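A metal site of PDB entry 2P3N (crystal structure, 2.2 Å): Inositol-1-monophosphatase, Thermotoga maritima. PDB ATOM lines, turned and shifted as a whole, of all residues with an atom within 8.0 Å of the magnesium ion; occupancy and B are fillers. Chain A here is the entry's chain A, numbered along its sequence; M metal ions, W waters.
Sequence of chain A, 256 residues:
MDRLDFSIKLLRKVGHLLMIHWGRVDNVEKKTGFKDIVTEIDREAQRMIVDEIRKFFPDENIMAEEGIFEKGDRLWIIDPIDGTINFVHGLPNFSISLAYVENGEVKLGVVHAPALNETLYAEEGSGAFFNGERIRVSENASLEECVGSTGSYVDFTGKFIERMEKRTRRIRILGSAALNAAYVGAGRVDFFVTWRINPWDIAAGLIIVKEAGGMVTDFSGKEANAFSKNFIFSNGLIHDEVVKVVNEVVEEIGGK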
ATOM      1  N   LYS A  31      22.734 -14.241 -31.469  1.00  0.00           N
ATOM      2  CA  LYS A  31      21.764 -15.044 -30.721  1.00  0.00           C
ATOM      3  C   LYS A  31      21.104 -16.077 -31.634  1.00  0.00           C
ATOM      4  O   LYS A  31      21.054 -17.259 -31.311  1.00  0.00           O
ATOM      5  CB  LYS A  31      20.718 -14.141 -30.041  1.00  0.00           C
ATOM      6  CG  LYS A  31      21.280 -13.363 -28.856  1.00  0.00           C
ATOM      7  CD  LYS A  31      20.359 -12.259 -28.359  1.00  0.00           C
ATOM      8  CE  LYS A  31      19.162 -12.781 -27.584  1.00  0.00           C
ATOM      9  NZ  LYS A  31      18.310 -11.667 -27.066  1.00  0.00           N
ATOM     10  N   ASP A  36      20.511 -10.602 -35.327  1.00  0.00           N
ATOM     11  CA  ASP A  36      19.991 -10.672 -33.968  1.00  0.00           C
ATOM     12  C   ASP A  36      21.137 -10.924 -32.989  1.00  0.00           C
ATOM     13  O   ASP A  36      21.442 -12.068 -32.636  1.00  0.00           O
ATOM     14  CB  ASP A  36      18.958 -11.788 -33.868  1.00  0.00           C
ATOM     15  CG  ASP A  36      18.521 -12.040 -32.463  1.00  0.00           C
ATOM     16  OD1 ASP A  36      18.323 -11.059 -31.721  1.00  0.00           O
ATOM     17  OD2 ASP A  36      18.371 -13.227 -32.089  1.00  0.00           O
ATOM     18  N   ILE A  37      21.759  -9.832 -32.554  1.00  0.00           N
ATOM     19  CA  ILE A  37      22.908  -9.907 -31.655  1.00  0.00           C
ATOM     20  C   ILE A  37      22.662  -9.375 -30.245  1.00  0.00           C
ATOM     21  O   ILE A  37      21.658  -8.724 -29.948  1.00  0.00           O
ATOM     22  CB  ILE A  37      24.100  -9.130 -32.228  1.00  0.00           C
ATOM     23  CG1 ILE A  37      23.694  -7.669 -32.438  1.00  0.00           C
ATOM     24  CG2 ILE A  37      24.564  -9.772 -33.529  1.00  0.00           C
ATOM     25  CD1 ILE A  37      24.850  -6.732 -32.694  1.00  0.00           C
ATOM     26  N   VAL A  38      23.617  -9.657 -29.375  1.00  0.00           N
ATOM     27  CA  VAL A  38      23.560  -9.207 -27.990  1.00  0.00           C
ATOM     28  C   VAL A  38      25.015  -8.988 -27.588  1.00  0.00           C
ATOM     29  O   VAL A  38      25.930  -9.579 -28.190  1.00  0.00           O
ATOM     30  CB  VAL A  38      22.891 -10.266 -27.062  1.00  0.00           C
ATOM     31  CG1 VAL A  38      23.697 -11.568 -27.072  1.00  0.00           C
ATOM     32  CG2 VAL A  38      22.769  -9.713 -25.648  1.00  0.00           C
ATOM     33  N   ASP A  42      24.538  -5.338 -22.860  1.00  0.00           N
ATOM     34  CA  ASP A  42      23.094  -5.545 -22.822  1.00  0.00           C
ATOM     35  C   ASP A  42      22.805  -6.169 -21.445  1.00  0.00           C
ATOM     36  O   ASP A  42      21.885  -5.751 -20.732  1.00  0.00           O
ATOM     37  CB  ASP A  42      22.643  -6.533 -23.920  1.00  0.00           C
ATOM     38  CG  ASP A  42      22.723  -5.944 -25.337  1.00  0.00           C
ATOM     39  OD1 ASP A  42      21.653  -5.673 -25.938  1.00  0.00           O
ATOM     40  OD2 ASP A  42      23.833  -5.761 -25.858  1.00  0.00           O
ATOM     41  N   GLN A  46      21.132  -4.777 -18.041  1.00  0.00           N
ATOM     42  CA  GLN A  46      19.986  -5.499 -17.524  1.00  0.00           C
ATOM     43  C   GLN A  46      20.154  -5.834 -16.050  1.00  0.00           C
ATOM     44  O   GLN A  46      19.187  -5.815 -15.294  1.00  0.00           O
ATOM     45  CB  GLN A  46      19.763  -6.781 -18.297  1.00  0.00           C
ATOM     46  CG  GLN A  46      18.415  -7.397 -18.011  1.00  0.00           C
ATOM     47  CD  GLN A  46      18.218  -8.699 -18.744  1.00  0.00           C
ATOM     48  OE1 GLN A  46      18.496  -9.770 -18.198  1.00  0.00           O
ATOM     49  NE2 GLN A  46      17.746  -8.624 -19.994  1.00  0.00           N
ATOM     50  N   GLU A  65      14.480  -9.128 -21.774  1.00  0.00           N
ATOM     51  CA  GLU A  65      14.941  -9.721 -23.021  1.00  0.00           C
ATOM     52  C   GLU A  65      16.039 -10.748 -22.822  1.00  0.00           C
ATOM     53  O   GLU A  65      15.868 -11.922 -23.133  1.00  0.00           O
ATOM     54  CB  GLU A  65      15.459  -8.640 -23.975  1.00  0.00           C
ATOM     55  CG  GLU A  65      16.277  -9.224 -25.102  1.00  0.00           C
ATOM     56  CD  GLU A  65      16.372  -8.307 -26.273  1.00  0.00           C
ATOM     57  OE1 GLU A  65      16.611  -7.099 -26.062  1.00  0.00           O
ATOM     58  OE2 GLU A  65      16.229  -8.801 -27.412  1.00  0.00           O
ATOM     59  N   GLU A  66      17.160 -10.311 -22.297  1.00  0.00           N
ATOM     60  CA  GLU A  66      18.293 -11.173 -22.088  1.00  0.00           C
ATOM     61  C   GLU A  66      18.152 -12.190 -20.957  1.00  0.00           C
ATOM     62  O   GLU A  66      18.770 -12.029 -19.904  1.00  0.00           O
ATOM     63  CB  GLU A  66      19.549 -10.320 -21.857  1.00  0.00           C
ATOM     64  CG  GLU A  66      20.404 -10.121 -23.093  1.00  0.00           C
ATOM     65  CD  GLU A  66      19.690  -9.389 -24.199  1.00  0.00           C
ATOM     66  OE1 GLU A  66      19.416  -8.184 -24.022  1.00  0.00           O
ATOM     67  OE2 GLU A  66      19.409 -10.007 -25.242  1.00  0.00           O
ATOM     68  N   ILE A  78      11.486  -5.567 -19.295  1.00  0.00           N
ATOM     69  CA  ILE A  78      12.714  -4.830 -19.551  1.00  0.00           C
ATOM     70  C   ILE A  78      13.443  -5.156 -20.833  1.00  0.00           C
ATOM     71  O   ILE A  78      13.632  -6.311 -21.177  1.00  0.00           O
ATOM     72  CB  ILE A  78      13.705  -5.084 -18.390  1.00  0.00           C
ATOM     73  CG1 ILE A  78      13.044  -4.664 -17.072  1.00  0.00           C
ATOM     74  CG2 ILE A  78      15.033  -4.375 -18.647  1.00  0.00           C
ATOM     75  CD1 ILE A  78      13.677  -5.308 -15.866  1.00  0.00           C
ATOM     76  N   ASP A  79      13.857  -4.117 -21.537  1.00  0.00           N
ATOM     77  CA  ASP A  79      14.680  -4.313 -22.714  1.00  0.00           C
ATOM     78  C   ASP A  79      15.917  -3.471 -22.381  1.00  0.00           C
ATOM     79  O   ASP A  79      15.891  -2.245 -22.480  1.00  0.00           O
ATOM     80  CB  ASP A  79      14.010  -3.822 -23.994  1.00  0.00           C
ATOM     81  CG  ASP A  79      14.791  -4.245 -25.240  1.00  0.00           C
ATOM     82  OD1 ASP A  79      14.202  -4.352 -26.333  1.00  0.00           O
ATOM     83  OD2 ASP A  79      16.010  -4.474 -25.113  1.00  0.00           O
ATOM     84  N   PRO A  80      17.000  -4.136 -21.944  1.00  0.00           N
ATOM     85  CA  PRO A  80      18.236  -3.438 -21.601  1.00  0.00           C
ATOM     86  C   PRO A  80      18.766  -2.533 -22.723  1.00  0.00           C
ATOM     87  O   PRO A  80      19.260  -1.443 -22.453  1.00  0.00           O
ATOM     88  CB  PRO A  80      19.187  -4.591 -21.238  1.00  0.00           C
ATOM     89  CG  PRO A  80      18.656  -5.758 -22.065  1.00  0.00           C
ATOM     90  CD  PRO A  80      17.180  -5.598 -21.872  1.00  0.00           C
ATOM     91  N   ILE A  81      18.674  -2.979 -23.972  1.00  0.00           N
ATOM     92  CA  ILE A  81      19.113  -2.158 -25.093  1.00  0.00           C
ATOM     93  C   ILE A  81      18.260  -2.459 -26.294  1.00  0.00           C
ATOM     94  O   ILE A  81      18.430  -3.492 -26.922  1.00  0.00           O
ATOM     95  CB  ILE A  81      20.584  -2.405 -25.521  1.00  0.00           C
ATOM     96  CG1 ILE A  81      21.553  -2.044 -24.386  1.00  0.00           C
ATOM     97  CG2 ILE A  81      20.898  -1.557 -26.750  1.00  0.00           C
ATOM     98  CD1 ILE A  81      23.013  -2.278 -24.707  1.00  0.00           C
ATOM     99  N   ASP A  82      17.328  -1.561 -26.588  1.00  0.00           N
ATOM    100  CA  ASP A  82      16.469  -1.763 -27.745  1.00  0.00           C
ATOM    101  C   ASP A  82      17.175  -1.072 -28.914  1.00  0.00           C
ATOM    102  O   ASP A  82      17.171   0.147 -29.018  1.00  0.00           O
ATOM    103  CB  ASP A  82      15.084  -1.147 -27.492  1.00  0.00           C
ATOM    104  CG  ASP A  82      14.120  -1.394 -28.641  1.00  0.00           C
ATOM    105  OD1 ASP A  82      12.932  -1.008 -28.513  1.00  0.00           O
ATOM    106  OD2 ASP A  82      14.538  -1.957 -29.671  1.00  0.00           O
ATOM    107  N   GLY A  83      17.800  -1.862 -29.774  1.00  0.00           N
ATOM    108  CA  GLY A  83      18.525  -1.294 -30.892  1.00  0.00           C
ATOM    109  C   GLY A  83      20.005  -1.585 -30.688  1.00  0.00           C
ATOM    110  O   GLY A  83      20.856  -0.710 -30.867  1.00  0.00           O
ATOM    111  N   THR A  84      20.296  -2.821 -30.302  1.00  0.00           N
ATOM    112  CA  THR A  84      21.663  -3.254 -30.036  1.00  0.00           C
ATOM    113  C   THR A  84      22.602  -3.105 -31.244  1.00  0.00           C
ATOM    114  O   THR A  84      23.805  -2.854 -31.074  1.00  0.00           O
ATOM    115  CB  THR A  84      21.679  -4.730 -29.554  1.00  0.00           C
ATOM    116  OG1 THR A  84      20.810  -4.863 -28.422  1.00  0.00           O
ATOM    117  CG2 THR A  84      23.084  -5.136 -29.157  1.00  0.00           C
ATOM    118  N   ILE A  85      22.047  -3.240 -32.447  1.00  0.00           N
ATOM    119  CA  ILE A  85      22.857  -3.101 -33.659  1.00  0.00           C
ATOM    120  C   ILE A  85      23.334  -1.662 -33.764  1.00  0.00           C
ATOM    121  O   ILE A  85      24.512  -1.396 -33.961  1.00  0.00           O
ATOM    122  CB  ILE A  85      22.044  -3.482 -34.918  1.00  0.00           C
ATOM    123  CG1 ILE A  85      21.774  -4.989 -34.910  1.00  0.00           C
ATOM    124  CG2 ILE A  85      22.783  -3.044 -36.172  1.00  0.00           C
ATOM    125  CD1 ILE A  85      20.847  -5.459 -36.013  1.00  0.00           C
ATOM    126  N   SER A  95      17.646   2.695 -27.202  1.00  0.00           N
ATOM    127  CA  SER A  95      17.015   3.101 -25.963  1.00  0.00           C
ATOM    128  C   SER A  95      16.897   1.978 -24.955  1.00  0.00           C
ATOM    129  O   SER A  95      17.223   0.823 -25.241  1.00  0.00           O
ATOM    130  CB  SER A  95      15.632   3.671 -26.263  1.00  0.00           C
ATOM    131  OG  SER A  95      14.871   2.766 -27.047  1.00  0.00           O
ATOM    132  N   ILE A  96      16.445   2.338 -23.757  1.00  0.00           N
ATOM    133  CA  ILE A  96      16.222   1.388 -22.671  1.00  0.00           C
ATOM    134  C   ILE A  96      14.728   1.447 -22.430  1.00  0.00           C
ATOM    135  O   ILE A  96      14.150   2.525 -22.343  1.00  0.00           O
ATOM    136  CB  ILE A  96      16.907   1.799 -21.360  1.00  0.00           C
ATOM    137  CG1 ILE A  96      18.393   2.111 -21.601  1.00  0.00           C
ATOM    138  CG2 ILE A  96      16.810   0.658 -20.364  1.00  0.00           C
ATOM    139  CD1 ILE A  96      19.123   2.500 -20.298  1.00  0.00           C
ATOM    140  N   SER A  97      14.080   0.301 -22.316  1.00  0.00           N
ATOM    141  CA  SER A  97      12.648   0.318 -22.106  1.00  0.00           C
ATOM    142  C   SER A  97      12.227  -0.415 -20.839  1.00  0.00           C
ATOM    143  O   SER A  97      12.766  -1.474 -20.506  1.00  0.00           O
ATOM    144  CB  SER A  97      11.959  -0.269 -23.337  1.00  0.00           C
ATOM    145  OG  SER A  97      10.591   0.114 -23.369  1.00  0.00           O
ATOM    146  N   TRP A 200       8.854  -6.962 -24.747  1.00  0.00           N
ATOM    147  CA  TRP A 200       9.787  -5.965 -24.200  1.00  0.00           C
ATOM    148  C   TRP A 200      10.106  -4.866 -25.197  1.00  0.00           C
ATOM    149  O   TRP A 200      10.653  -3.821 -24.826  1.00  0.00           O
ATOM    150  CB  TRP A 200      11.082  -6.622 -23.698  1.00  0.00           C
ATOM    151  CG  TRP A 200      11.733  -7.573 -24.638  1.00  0.00           C
ATOM    152  CD1 TRP A 200      12.509  -7.280 -25.734  1.00  0.00           C
ATOM    153  CD2 TRP A 200      11.712  -8.996 -24.538  1.00  0.00           C
ATOM    154  NE1 TRP A 200      12.964  -8.435 -26.312  1.00  0.00           N
ATOM    155  CE2 TRP A 200      12.493  -9.508 -25.606  1.00  0.00           C
ATOM    156  CE3 TRP A 200      11.102  -9.892 -23.660  1.00  0.00           C
ATOM    157  CZ2 TRP A 200      12.673 -10.874 -25.808  1.00  0.00           C
ATOM    158  CZ3 TRP A 200      11.293 -11.254 -23.855  1.00  0.00           C
ATOM    159  CH2 TRP A 200      12.077 -11.723 -24.922  1.00  0.00           C
ATOM    160  N   ASP A 201       9.756  -5.117 -26.465  1.00  0.00           N
ATOM    161  CA  ASP A 201       9.969  -4.181 -27.557  1.00  0.00           C
ATOM    162  C   ASP A 201       8.785  -3.224 -27.665  1.00  0.00           C
ATOM    163  O   ASP A 201       8.936  -2.103 -28.142  1.00  0.00           O
ATOM    164  CB  ASP A 201      10.107  -4.916 -28.895  1.00  0.00           C
ATOM    165  CG  ASP A 201      11.347  -5.789 -28.958  1.00  0.00           C
ATOM    166  OD1 ASP A 201      12.474  -5.261 -28.825  1.00  0.00           O
ATOM    167  OD2 ASP A 201      11.182  -7.019 -29.154  1.00  0.00           O
HETATM  168 MG    MG M   1      17.362  -5.225 -26.642  1.00  0.00          MG
HETATM  169  O   HOH W   1      18.463  -6.053 -28.000  1.00  0.00           O
HETATM  170  O   HOH W   2      18.995  -5.703 -25.150  1.00  0.00           O
HETATM  171  O   HOH W   3      16.037  -5.264 -28.284  1.00  0.00           O
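The side-chain hydroxyl of Thr 84 sits close to the backbone carbonyl oxygen of Ile 81 (3.1 Å).
The side-chain carboxylate of Glu 65 lies close to the indole nitrogen of Trp 200, at 3.5 Å.
The side-chain carboxylate (OE2) of Glu 65 lies within salt-bridge range of the side-chain amino group (NZ) of Lys 31, at 3.6 Å.
O of Ile 78 is in hydrogen-bond range of N of Glu 65.
N of Asp 79 is in hydrogen-bond range of O of Ser 97 (3.0 Å).
The backbone carbonyl oxygen (O) of Ser 95 sits at hydrogen-bond distance from the backbone NH (N) of Asp 82 (2.7 Å).
The side-chain hydroxyl of Thr 84 is in hydrogen-bond range of the side-chain carboxylate of Asp 42 (2.7 Å).
Asp 82 touches the magnesium ion (N to MG, 3.7 Å).
OG1 of Thr 84 touches the magnesium ion, at 3.9 Å.
Of the 21 residues printed, 5 come within 4 Å of the magnesium ion.
The magnesium ion is bound by water W1, O of Ile 81, OE1 of Glu 65, water W3, OD2 of Asp 79 and water W2.
The magnesium ion has six donor atoms within binding distance.
Water W2 lies within hydrogen-bond range of OE1 of Glu 66 (2.8 Å), OD1 of Asp 42 (2.8 Å) and N of Ile 81 (3.0 Å).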
